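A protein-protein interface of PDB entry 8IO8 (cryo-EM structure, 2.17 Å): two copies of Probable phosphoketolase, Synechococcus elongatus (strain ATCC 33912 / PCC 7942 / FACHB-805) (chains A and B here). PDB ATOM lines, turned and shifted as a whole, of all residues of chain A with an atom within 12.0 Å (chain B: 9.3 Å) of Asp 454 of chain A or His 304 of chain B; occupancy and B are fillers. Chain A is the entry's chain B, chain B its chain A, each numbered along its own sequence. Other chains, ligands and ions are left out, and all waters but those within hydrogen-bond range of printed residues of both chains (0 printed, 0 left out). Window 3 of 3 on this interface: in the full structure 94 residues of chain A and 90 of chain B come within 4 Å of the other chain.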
ATOM      1  N   ALA A 429      -9.647 -15.970  36.780  1.00  0.00           N
ATOM      2  CA  ALA A 429      -8.264 -16.126  36.345  1.00  0.00           C
ATOM      3  C   ALA A 429      -7.302 -15.431  37.299  1.00  0.00           C
ATOM      4  O   ALA A 429      -6.226 -15.960  37.599  1.00  0.00           O
ATOM      5  CB  ALA A 429      -8.095 -15.590  34.925  1.00  0.00           C
ATOM      6  N   ASP A 434      -8.259 -21.174  37.868  1.00  0.00           N
ATOM      7  CA  ASP A 434      -8.389 -21.587  36.473  1.00  0.00           C
ATOM      8  C   ASP A 434      -8.718 -23.066  36.336  1.00  0.00           C
ATOM      9  O   ASP A 434      -9.168 -23.499  35.270  1.00  0.00           O
ATOM     10  CB  ASP A 434      -7.103 -21.276  35.712  1.00  0.00           C
ATOM     11  CG  ASP A 434      -6.691 -19.833  35.841  1.00  0.00           C
ATOM     12  OD1 ASP A 434      -7.363 -19.100  36.591  1.00  0.00           O
ATOM     13  OD2 ASP A 434      -5.700 -19.431  35.196  1.00  0.00           O
ATOM     14  N   TYR A 437     -11.861 -24.330  34.687  1.00  0.00           N
ATOM     15  CA  TYR A 437     -12.024 -24.276  33.241  1.00  0.00           C
ATOM     16  C   TYR A 437     -11.725 -25.607  32.567  1.00  0.00           C
ATOM     17  O   TYR A 437     -11.961 -25.736  31.362  1.00  0.00           O
ATOM     18  CB  TYR A 437     -11.135 -23.184  32.649  1.00  0.00           C
ATOM     19  CG  TYR A 437     -11.507 -21.795  33.106  1.00  0.00           C
ATOM     20  CD1 TYR A 437     -12.827 -21.466  33.377  1.00  0.00           C
ATOM     21  CD2 TYR A 437     -10.540 -20.817  33.278  1.00  0.00           C
ATOM     22  CE1 TYR A 437     -13.173 -20.202  33.799  1.00  0.00           C
ATOM     23  CE2 TYR A 437     -10.877 -19.550  33.700  1.00  0.00           C
ATOM     24  CZ  TYR A 437     -12.195 -19.247  33.960  1.00  0.00           C
ATOM     25  OH  TYR A 437     -12.534 -17.984  34.382  1.00  0.00           O
ATOM     26  N   GLU A 438     -11.211 -26.588  33.307  1.00  0.00           N
ATOM     27  CA  GLU A 438     -10.924 -27.894  32.730  1.00  0.00           C
ATOM     28  C   GLU A 438     -12.183 -28.719  32.493  1.00  0.00           C
ATOM     29  O   GLU A 438     -12.148 -29.656  31.690  1.00  0.00           O
ATOM     30  CB  GLU A 438      -9.961 -28.659  33.635  1.00  0.00           C
ATOM     31  CG  GLU A 438      -8.670 -27.912  33.914  1.00  0.00           C
ATOM     32  CD  GLU A 438      -7.813 -28.593  34.958  1.00  0.00           C
ATOM     33  OE1 GLU A 438      -8.180 -29.700  35.403  1.00  0.00           O
ATOM     34  OE2 GLU A 438      -6.770 -28.020  35.335  1.00  0.00           O
ATOM     35  N   THR A 440     -15.641 -26.944  32.796  1.00  0.00           N
ATOM     36  CA  THR A 440     -16.659 -26.024  32.310  1.00  0.00           C
ATOM     37  C   THR A 440     -16.011 -24.768  31.746  1.00  0.00           C
ATOM     38  O   THR A 440     -14.793 -24.725  31.553  1.00  0.00           O
ATOM     39  CB  THR A 440     -17.641 -25.659  33.424  1.00  0.00           C
ATOM     40  OG1 THR A 440     -18.675 -24.824  32.894  1.00  0.00           O
ATOM     41  CG2 THR A 440     -16.929 -24.919  34.543  1.00  0.00           C
ATOM     42  N   SER A 441     -16.817 -23.751  31.466  1.00  0.00           N
ATOM     43  CA  SER A 441     -16.312 -22.484  30.965  1.00  0.00           C
ATOM     44  C   SER A 441     -17.164 -21.370  31.558  1.00  0.00           C
ATOM     45  O   SER A 441     -17.962 -21.592  32.473  1.00  0.00           O
ATOM     46  CB  SER A 441     -16.317 -22.470  29.432  1.00  0.00           C
ATOM     47  OG  SER A 441     -17.621 -22.699  28.942  1.00  0.00           O
ATOM     48  N   LYS A 442     -16.992 -20.162  31.036  1.00  0.00           N
ATOM     49  CA  LYS A 442     -17.766 -19.007  31.461  1.00  0.00           C
ATOM     50  C   LYS A 442     -18.937 -18.817  30.511  1.00  0.00           C
ATOM     51  O   LYS A 442     -18.765 -18.879  29.289  1.00  0.00           O
ATOM     52  CB  LYS A 442     -16.896 -17.752  31.498  1.00  0.00           C
ATOM     53  CG  LYS A 442     -15.906 -17.732  32.644  1.00  0.00           C
ATOM     54  CD  LYS A 442     -14.846 -16.670  32.441  1.00  0.00           C
ATOM     55  CE  LYS A 442     -13.986 -16.985  31.231  1.00  0.00           C
ATOM     56  NZ  LYS A 442     -12.933 -15.962  31.017  1.00  0.00           N
ATOM     57  N   ARG A 448     -19.344 -14.087  19.622  1.00  0.00           N
ATOM     58  CA  ARG A 448     -18.071 -14.755  19.834  1.00  0.00           C
ATOM     59  C   ARG A 448     -17.192 -14.594  18.604  1.00  0.00           C
ATOM     60  O   ARG A 448     -17.681 -14.508  17.475  1.00  0.00           O
ATOM     61  CB  ARG A 448     -18.262 -16.241  20.141  1.00  0.00           C
ATOM     62  CG  ARG A 448     -19.035 -16.512  21.415  1.00  0.00           C
ATOM     63  CD  ARG A 448     -18.950 -17.976  21.787  1.00  0.00           C
ATOM     64  NE  ARG A 448     -17.567 -18.394  21.971  1.00  0.00           N
ATOM     65  CZ  ARG A 448     -17.186 -19.644  22.197  1.00  0.00           C
ATOM     66  NH1 ARG A 448     -18.063 -20.631  22.267  1.00  0.00           N
ATOM     67  NH2 ARG A 448     -15.893 -19.908  22.355  1.00  0.00           N
ATOM     68  N   ILE A 449     -15.888 -14.553  18.837  1.00  0.00           N
ATOM     69  CA  ILE A 449     -14.907 -14.401  17.766  1.00  0.00           C
ATOM     70  C   ILE A 449     -13.947 -15.577  17.855  1.00  0.00           C
ATOM     71  O   ILE A 449     -13.785 -16.184  18.927  1.00  0.00           O
ATOM     72  CB  ILE A 449     -14.173 -13.043  17.848  1.00  0.00           C
ATOM     73  CG1 ILE A 449     -13.392 -12.929  19.157  1.00  0.00           C
ATOM     74  CG2 ILE A 449     -15.162 -11.896  17.722  1.00  0.00           C
ATOM     75  CD1 ILE A 449     -12.621 -11.640  19.284  1.00  0.00           C
ATOM     76  N   PRO A 450     -13.305 -15.945  16.743  1.00  0.00           N
ATOM     77  CA  PRO A 450     -12.368 -17.081  16.783  1.00  0.00           C
ATOM     78  C   PRO A 450     -11.176 -16.862  17.698  1.00  0.00           C
ATOM     79  O   PRO A 450     -10.538 -17.842  18.098  1.00  0.00           O
ATOM     80  CB  PRO A 450     -11.934 -17.232  15.318  1.00  0.00           C
ATOM     81  CG  PRO A 450     -12.236 -15.915  14.689  1.00  0.00           C
ATOM     82  CD  PRO A 450     -13.462 -15.415  15.379  1.00  0.00           C
ATOM     83  N   GLU A 451     -10.851 -15.614  18.039  1.00  0.00           N
ATOM     84  CA  GLU A 451      -9.778 -15.360  18.993  1.00  0.00           C
ATOM     85  C   GLU A 451     -10.128 -15.836  20.396  1.00  0.00           C
ATOM     86  O   GLU A 451      -9.225 -16.018  21.218  1.00  0.00           O
ATOM     87  CB  GLU A 451      -9.435 -13.869  19.025  1.00  0.00           C
ATOM     88  CG  GLU A 451      -8.759 -13.343  17.765  1.00  0.00           C
ATOM     89  CD  GLU A 451      -9.726 -13.143  16.611  1.00  0.00           C
ATOM     90  OE1 GLU A 451     -10.951 -13.246  16.829  1.00  0.00           O
ATOM     91  OE2 GLU A 451      -9.259 -12.883  15.482  1.00  0.00           O
ATOM     92  N   ASP A 452     -11.412 -16.039  20.688  1.00  0.00           N
ATOM     93  CA  ASP A 452     -11.833 -16.537  21.990  1.00  0.00           C
ATOM     94  C   ASP A 452     -11.547 -18.019  22.181  1.00  0.00           C
ATOM     95  O   ASP A 452     -11.679 -18.519  23.301  1.00  0.00           O
ATOM     96  CB  ASP A 452     -13.329 -16.282  22.197  1.00  0.00           C
ATOM     97  CG  ASP A 452     -13.656 -14.811  22.337  1.00  0.00           C
ATOM     98  OD1 ASP A 452     -12.788 -14.051  22.812  1.00  0.00           O
ATOM     99  OD2 ASP A 452     -14.783 -14.417  21.976  1.00  0.00           O
ATOM    100  N   GLU A 453     -11.169 -18.732  21.121  1.00  0.00           N
ATOM    101  CA  GLU A 453     -10.920 -20.162  21.230  1.00  0.00           C
ATOM    102  C   GLU A 453      -9.578 -20.485  21.868  1.00  0.00           C
ATOM    103  O   GLU A 453      -9.372 -21.623  22.297  1.00  0.00           O
ATOM    104  CB  GLU A 453     -10.998 -20.813  19.848  1.00  0.00           C
ATOM    105  CG  GLU A 453     -12.270 -20.491  19.088  1.00  0.00           C
ATOM    106  CD  GLU A 453     -13.519 -20.937  19.822  1.00  0.00           C
ATOM    107  OE1 GLU A 453     -13.478 -21.992  20.489  1.00  0.00           O
ATOM    108  OE2 GLU A 453     -14.543 -20.226  19.737  1.00  0.00           O
ATOM    109  N   ASP A 454      -8.665 -19.516  21.943  1.00  0.00           N
ATOM    110  CA  ASP A 454      -7.342 -19.788  22.494  1.00  0.00           C
ATOM    111  C   ASP A 454      -7.405 -19.959  24.008  1.00  0.00           C
ATOM    112  O   ASP A 454      -7.083 -21.027  24.540  1.00  0.00           O
ATOM    113  CB  ASP A 454      -6.375 -18.665  22.113  1.00  0.00           C
ATOM    114  CG  ASP A 454      -4.928 -19.018  22.402  1.00  0.00           C
ATOM    115  OD1 ASP A 454      -4.658 -20.170  22.799  1.00  0.00           O
ATOM    116  OD2 ASP A 454      -4.055 -18.142  22.229  1.00  0.00           O
ATOM    117  N   GLY A 455      -7.823 -18.916  24.718  1.00  0.00           N
ATOM    118  CA  GLY A 455      -7.928 -18.987  26.159  1.00  0.00           C
ATOM    119  C   GLY A 455      -9.129 -18.236  26.692  1.00  0.00           C
ATOM    120  O   GLY A 455      -9.157 -17.847  27.863  1.00  0.00           O
ATOM    121  N   GLY A 456     -10.124 -18.016  25.833  1.00  0.00           N
ATOM    122  CA  GLY A 456     -11.297 -17.267  26.251  1.00  0.00           C
ATOM    123  C   GLY A 456     -12.122 -17.992  27.297  1.00  0.00           C
ATOM    124  O   GLY A 456     -12.624 -17.372  28.238  1.00  0.00           O
ATOM    125  N   HIS A 457     -12.273 -19.310  27.147  1.00  0.00           N
ATOM    126  CA  HIS A 457     -13.086 -20.137  28.039  1.00  0.00           C
ATOM    127  C   HIS A 457     -14.524 -19.620  28.105  1.00  0.00           C
ATOM    128  O   HIS A 457     -15.059 -19.312  29.170  1.00  0.00           O
ATOM    129  CB  HIS A 457     -12.464 -20.220  29.437  1.00  0.00           C
ATOM    130  CG  HIS A 457     -11.079 -20.783  29.449  1.00  0.00           C
ATOM    131  ND1 HIS A 457     -10.788 -22.052  28.997  1.00  0.00           N
ATOM    132  CD2 HIS A 457      -9.904 -20.252  29.861  1.00  0.00           C
ATOM    133  CE1 HIS A 457      -9.493 -22.277  29.128  1.00  0.00           C
ATOM    134  NE2 HIS A 457      -8.934 -21.200  29.650  1.00  0.00           N
ATOM    135  N   LEU A 458     -15.145 -19.530  26.934  1.00  0.00           N
ATOM    136  CA  LEU A 458     -16.509 -19.045  26.799  1.00  0.00           C
ATOM    137  C   LEU A 458     -17.366 -20.098  26.114  1.00  0.00           C
ATOM    138  O   LEU A 458     -16.948 -20.705  25.124  1.00  0.00           O
ATOM    139  CB  LEU A 458     -16.562 -17.743  25.995  1.00  0.00           C
ATOM    140  CG  LEU A 458     -15.705 -16.569  26.463  1.00  0.00           C
ATOM    141  CD1 LEU A 458     -15.838 -15.415  25.494  1.00  0.00           C
ATOM    142  CD2 LEU A 458     -16.098 -16.137  27.863  1.00  0.00           C
ATOM    143  N   SER A 459     -18.562 -20.316  26.651  1.00  0.00           N
ATOM    144  CA  SER A 459     -19.550 -21.168  26.006  1.00  0.00           C
ATOM    145  C   SER A 459     -20.922 -20.781  26.531  1.00  0.00           C
ATOM    146  O   SER A 459     -21.046 -20.123  27.565  1.00  0.00           O
ATOM    147  CB  SER A 459     -19.276 -22.654  26.253  1.00  0.00           C
ATOM    148  OG  SER A 459     -19.426 -22.982  27.621  1.00  0.00           O
ATOM    149  N   TYR B 213     -12.197  -5.715  25.811  1.00  0.00           N
ATOM    150  CA  TYR B 213     -11.866  -6.601  26.915  1.00  0.00           C
ATOM    151  C   TYR B 213     -11.685  -5.774  28.175  1.00  0.00           C
ATOM    152  O   TYR B 213     -11.472  -4.562  28.118  1.00  0.00           O
ATOM    153  CB  TYR B 213     -10.599  -7.415  26.623  1.00  0.00           C
ATOM    154  CG  TYR B 213     -10.704  -8.288  25.396  1.00  0.00           C
ATOM    155  CD1 TYR B 213     -11.199  -9.579  25.481  1.00  0.00           C
ATOM    156  CD2 TYR B 213     -10.309  -7.819  24.153  1.00  0.00           C
ATOM    157  CE1 TYR B 213     -11.297 -10.377  24.365  1.00  0.00           C
ATOM    158  CE2 TYR B 213     -10.407  -8.610  23.033  1.00  0.00           C
ATOM    159  CZ  TYR B 213     -10.901  -9.888  23.144  1.00  0.00           C
ATOM    160  OH  TYR B 213     -10.997 -10.682  22.028  1.00  0.00           O
ATOM    161  N   PRO B 298       3.431  -5.568  21.794  1.00  0.00           N
ATOM    162  CA  PRO B 298       3.829  -6.789  21.086  1.00  0.00           C
ATOM    163  C   PRO B 298       2.622  -7.507  20.506  1.00  0.00           C
ATOM    164  O   PRO B 298       1.577  -7.621  21.148  1.00  0.00           O
ATOM    165  CB  PRO B 298       4.510  -7.624  22.175  1.00  0.00           C
ATOM    166  CG  PRO B 298       4.894  -6.645  23.226  1.00  0.00           C
ATOM    167  CD  PRO B 298       3.845  -5.588  23.205  1.00  0.00           C
ATOM    168  N   ALA B 299       2.777  -7.997  19.276  1.00  0.00           N
ATOM    169  CA  ALA B 299       1.661  -8.649  18.601  1.00  0.00           C
ATOM    170  C   ALA B 299       1.326  -9.984  19.252  1.00  0.00           C
ATOM    171  O   ALA B 299       0.163 -10.260  19.565  1.00  0.00           O
ATOM    172  CB  ALA B 299       1.981  -8.836  17.120  1.00  0.00           C
ATOM    173  N   THR B 300       2.335 -10.825  19.470  1.00  0.00           N
ATOM    174  CA  THR B 300       2.138 -12.142  20.055  1.00  0.00           C
ATOM    175  C   THR B 300       3.248 -12.432  21.050  1.00  0.00           C
ATOM    176  O   THR B 300       4.411 -12.103  20.806  1.00  0.00           O
ATOM    177  CB  THR B 300       2.114 -13.249  18.991  1.00  0.00           C
ATOM    178  OG1 THR B 300       3.306 -13.180  18.200  1.00  0.00           O
ATOM    179  CG2 THR B 300       0.896 -13.118  18.090  1.00  0.00           C
ATOM    180  N   ILE B 301       2.880 -13.049  22.168  1.00  0.00           N
ATOM    181  CA  ILE B 301       3.829 -13.534  23.160  1.00  0.00           C
ATOM    182  C   ILE B 301       3.528 -15.003  23.412  1.00  0.00           C
ATOM    183  O   ILE B 301       2.381 -15.361  23.704  1.00  0.00           O
ATOM    184  CB  ILE B 301       3.755 -12.733  24.474  1.00  0.00           C
ATOM    185  CG1 ILE B 301       4.084 -11.260  24.226  1.00  0.00           C
ATOM    186  CG2 ILE B 301       4.697 -13.318  25.508  1.00  0.00           C
ATOM    187  CD1 ILE B 301       5.458 -11.033  23.653  1.00  0.00           C
ATOM    188  N   LYS B 302       4.552 -15.850  23.288  1.00  0.00           N
ATOM    189  CA  LYS B 302       4.423 -17.295  23.479  1.00  0.00           C
ATOM    190  C   LYS B 302       3.402 -17.906  22.525  1.00  0.00           C
ATOM    191  O   LYS B 302       2.770 -18.916  22.841  1.00  0.00           O
ATOM    192  CB  LYS B 302       4.065 -17.639  24.928  1.00  0.00           C
ATOM    193  CG  LYS B 302       5.047 -17.118  25.959  1.00  0.00           C
ATOM    194  CD  LYS B 302       6.417 -17.741  25.780  1.00  0.00           C
ATOM    195  CE  LYS B 302       7.350 -17.344  26.911  1.00  0.00           C
ATOM    196  NZ  LYS B 302       8.704 -17.940  26.756  1.00  0.00           N
ATOM    197  N   GLY B 303       3.229 -17.301  21.354  1.00  0.00           N
ATOM    198  CA  GLY B 303       2.291 -17.797  20.372  1.00  0.00           C
ATOM    199  C   GLY B 303       0.850 -17.386  20.579  1.00  0.00           C
ATOM    200  O   GLY B 303      -0.005 -17.765  19.770  1.00  0.00           O
ATOM    201  N   HIS B 304       0.550 -16.625  21.624  1.00  0.00           N
ATOM    202  CA  HIS B 304      -0.803 -16.166  21.898  1.00  0.00           C
ATOM    203  C   HIS B 304      -0.950 -14.710  21.482  1.00  0.00           C
ATOM    204  O   HIS B 304      -0.013 -13.919  21.614  1.00  0.00           O
ATOM    205  CB  HIS B 304      -1.146 -16.314  23.379  1.00  0.00           C
ATOM    206  CG  HIS B 304      -1.000 -17.710  23.896  1.00  0.00           C
ATOM    207  ND1 HIS B 304      -0.843 -17.993  25.235  1.00  0.00           N
ATOM    208  CD2 HIS B 304      -0.991 -18.902  23.255  1.00  0.00           C
ATOM    209  CE1 HIS B 304      -0.740 -19.300  25.397  1.00  0.00           C
ATOM    210  NE2 HIS B 304      -0.827 -19.874  24.212  1.00  0.00           N
ATOM    211  N   VAL B 305      -2.135 -14.361  20.983  1.00  0.00           N
ATOM    212  CA  VAL B 305      -2.409 -12.987  20.590  1.00  0.00           C
ATOM    213  C   VAL B 305      -2.448 -12.107  21.831  1.00  0.00           C
ATOM    214  O   VAL B 305      -3.142 -12.413  22.808  1.00  0.00           O
ATOM    215  CB  VAL B 305      -3.727 -12.907  19.806  1.00  0.00           C
ATOM    216  CG1 VAL B 305      -4.124 -11.463  19.577  1.00  0.00           C
ATOM    217  CG2 VAL B 305      -3.593 -13.638  18.484  1.00  0.00           C
ATOM    218  N   VAL B 306      -1.697 -11.010  21.801  1.00  0.00           N
ATOM    219  CA  VAL B 306      -1.613 -10.076  22.916  1.00  0.00           C
ATOM    220  C   VAL B 306      -2.257  -8.738  22.570  1.00  0.00           C
ATOM    221  O   VAL B 306      -3.131  -8.257  23.289  1.00  0.00           O
ATOM    222  CB  VAL B 306      -0.148  -9.887  23.368  1.00  0.00           C
ATOM    223  CG1 VAL B 306      -0.071  -8.891  24.504  1.00  0.00           C
ATOM    224  CG2 VAL B 306       0.440 -11.215  23.789  1.00  0.00           C
ATOM    225  N   GLU B 307      -1.828  -8.121  21.472  1.00  0.00           N
ATOM    226  CA  GLU B 307      -2.447  -6.883  21.020  1.00  0.00           C
ATOM    227  C   GLU B 307      -3.876  -7.148  20.567  1.00  0.00           C
ATOM    228  O   GLU B 307      -4.136  -8.099  19.823  1.00  0.00           O
ATOM    229  CB  GLU B 307      -1.636  -6.268  19.883  1.00  0.00           C
ATOM    230  CG  GLU B 307      -2.341  -5.135  19.167  1.00  0.00           C
ATOM    231  CD  GLU B 307      -1.621  -4.717  17.905  1.00  0.00           C
ATOM    232  OE1 GLU B 307      -0.446  -5.102  17.734  1.00  0.00           O
ATOM    233  OE2 GLU B 307      -2.228  -3.998  17.083  1.00  0.00           O
ATOM    234  N   GLY B 308      -4.803  -6.303  21.008  1.00  0.00           N
ATOM    235  CA  GLY B 308      -6.201  -6.551  20.733  1.00  0.00           C
ATOM    236  C   GLY B 308      -6.784  -7.702  21.513  1.00  0.00           C
ATOM    237  O   GLY B 308      -7.783  -8.285  21.088  1.00  0.00           O
ATOM    238  N   SER B 309      -6.180  -8.050  22.644  1.00  0.00           N
ATOM    239  CA  SER B 309      -6.633  -9.158  23.466  1.00  0.00           C
ATOM    240  C   SER B 309      -6.602  -8.734  24.925  1.00  0.00           C
ATOM    241  O   SER B 309      -6.043  -7.695  25.282  1.00  0.00           O
ATOM    242  CB  SER B 309      -5.773 -10.407  23.252  1.00  0.00           C
ATOM    243  OG  SER B 309      -6.135 -11.437  24.152  1.00  0.00           O
ATOM    244  N   TRP B 310      -7.216  -9.557  25.773  1.00  0.00           N
ATOM    245  CA  TRP B 310      -7.185  -9.305  27.207  1.00  0.00           C
ATOM    246  C   TRP B 310      -5.815  -9.581  27.809  1.00  0.00           C
ATOM    247  O   TRP B 310      -5.553  -9.157  28.939  1.00  0.00           O
ATOM    248  CB  TRP B 310      -8.241 -10.159  27.910  1.00  0.00           C
ATOM    249  CG  TRP B 310      -8.104 -11.612  27.608  1.00  0.00           C
ATOM    250  CD1 TRP B 310      -8.738 -12.304  26.622  1.00  0.00           C
ATOM    251  CD2 TRP B 310      -7.267 -12.555  28.286  1.00  0.00           C
ATOM    252  NE1 TRP B 310      -8.354 -13.621  26.647  1.00  0.00           N
ATOM    253  CE2 TRP B 310      -7.451 -13.800  27.661  1.00  0.00           C
ATOM    254  CE3 TRP B 310      -6.384 -12.468  29.365  1.00  0.00           C
ATOM    255  CZ2 TRP B 310      -6.786 -14.949  28.075  1.00  0.00           C
ATOM    256  CZ3 TRP B 310      -5.725 -13.606  29.774  1.00  0.00           C
ATOM    257  CH2 TRP B 310      -5.928 -14.831  29.132  1.00  0.00           C
ATOM    258  N   ARG B 311      -4.941 -10.280  27.085  1.00  0.00           N
ATOM    259  CA  ARG B 311      -3.621 -10.610  27.605  1.00  0.00           C
ATOM    260  C   ARG B 311      -2.704  -9.402  27.710  1.00  0.00           C
ATOM    261  O   ARG B 311      -1.653  -9.498  28.352  1.00  0.00           O
ATOM    262  CB  ARG B 311      -2.971 -11.684  26.734  1.00  0.00           C
ATOM    263  CG  ARG B 311      -3.374 -13.097  27.114  1.00  0.00           C
ATOM    264  CD  ARG B 311      -2.749 -14.131  26.200  1.00  0.00           C
ATOM    265  NE  ARG B 311      -3.470 -14.243  24.938  1.00  0.00           N
ATOM    266  CZ  ARG B 311      -4.425 -15.131  24.700  1.00  0.00           C
ATOM    267  NH1 ARG B 311      -4.795 -16.010  25.615  1.00  0.00           N
ATOM    268  NH2 ARG B 311      -5.024 -15.135  23.513  1.00  0.00           N
ATOM    269  N   SER B 312      -3.067  -8.276  27.108  1.00  0.00           N
ATOM    270  CA  SER B 312      -2.278  -7.057  27.191  1.00  0.00           C
ATOM    271  C   SER B 312      -2.731  -6.139  28.318  1.00  0.00           C
ATOM    272  O   SER B 312      -2.200  -5.032  28.444  1.00  0.00           O
ATOM    273  CB  SER B 312      -2.333  -6.308  25.861  1.00  0.00           C
ATOM    274  OG  SER B 312      -3.665  -5.956  25.542  1.00  0.00           O
ATOM    275  N   PRO B 316       2.181  -7.254  28.711  1.00  0.00           N
ATOM    276  CA  PRO B 316       2.382  -8.283  27.681  1.00  0.00           C
ATOM    277  C   PRO B 316       3.439  -9.301  28.060  1.00  0.00           C
ATOM    278  O   PRO B 316       3.321 -10.474  27.687  1.00  0.00           O
ATOM    279  CB  PRO B 316       2.794  -7.465  26.451  1.00  0.00           C
ATOM    280  CG  PRO B 316       2.234  -6.109  26.702  1.00  0.00           C
ATOM    281  CD  PRO B 316       2.356  -5.898  28.176  1.00  0.00           C
ATOM    282  N   HIS B 326      12.539 -12.536  26.201  1.00  0.00           N
ATOM    283  CA  HIS B 326      11.541 -11.511  26.472  1.00  0.00           C
ATOM    284  C   HIS B 326      12.180 -10.147  26.686  1.00  0.00           C
ATOM    285  O   HIS B 326      11.576  -9.125  26.346  1.00  0.00           O
ATOM    286  CB  HIS B 326      10.692 -11.904  27.679  1.00  0.00           C
ATOM    287  CG  HIS B 326       9.538 -12.790  27.333  1.00  0.00           C
ATOM    288  ND1 HIS B 326       8.546 -13.106  28.234  1.00  0.00           N
ATOM    289  CD2 HIS B 326       9.215 -13.421  26.181  1.00  0.00           C
ATOM    290  CE1 HIS B 326       7.662 -13.896  27.653  1.00  0.00           C
ATOM    291  NE2 HIS B 326       8.045 -14.103  26.406  1.00  0.00           N
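OH of Tyr 213 of chain B touches CD1 of Ile 449 of chain A (3.3 Å). OD1 of Asp 452 of chain A touches OH of Tyr 213 of chain B, 3.9 Å away. His 304 of chain B touches Asp 454 of chain A (CD2 to OD2, 3.3 Å). Gly 455 of chain A touches Trp 310 of chain B (O to CZ2, 3.8 Å).
OG of Ser 309 of chain B sits close to N of Arg 311 of chain B, 3.4 Å away. The guanidinium group of Arg 311 of chain B sits at hydrogen-bond distance from the backbone carbonyl oxygen of Val 305 of chain B (2.8 Å). The backbone NH (N) of Ile 449 of chain A sits at hydrogen-bond distance from the side-chain carboxylate (OD2) of Asp 452 of chain A (3.3 Å).
No position is printed for both chains. Of the 5 pairs that touch across the chains among the printed residues, none has its exchanged pair printed and touching as well.
The guanidinium group (NH2) of Arg 311 of chain B lies within salt-bridge range of the side-chain carboxylate (OD2) of Asp 454 of chain A (3.4 Å).
Of the printed residues of chain B, Ile 449 of chain A touches Tyr 213 (3.3 Å). Of the printed residues of chain B, Asp 452 of chain A touches Tyr 213 (3.9 Å). Asp 454 of chain A touches just these residues of chain B: His 304 (3.3 Å) and Arg 311 (3.4 Å). Of chain B, only Trp 310 (3.8 Å) comes within 4 Å of Gly 455 of chain A. No residue of chain A comes within 4 Å of Ala 299 of chain B. No residue of chain A comes within 4 Å of Thr 300 of chain B. Gly 303 of chain B touches none of the printed residues of chain A. His 304 of chain B touches one residue of chain A. No residue of chain A comes within 4 Å of Val 305 of chain B.
Of the 19 printed residues of chain A, 4 touch a printed residue of chain B. Hydrophobic or aromatic side chains of chain A within 4 Å of the printed part of chain B: Ile 449. Printed residues of chain B that touch a printed residue of chain A: Tyr 213, His 304, Trp 310 and Arg 311. Among the printed residues, 5 pairs touch across the chains.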
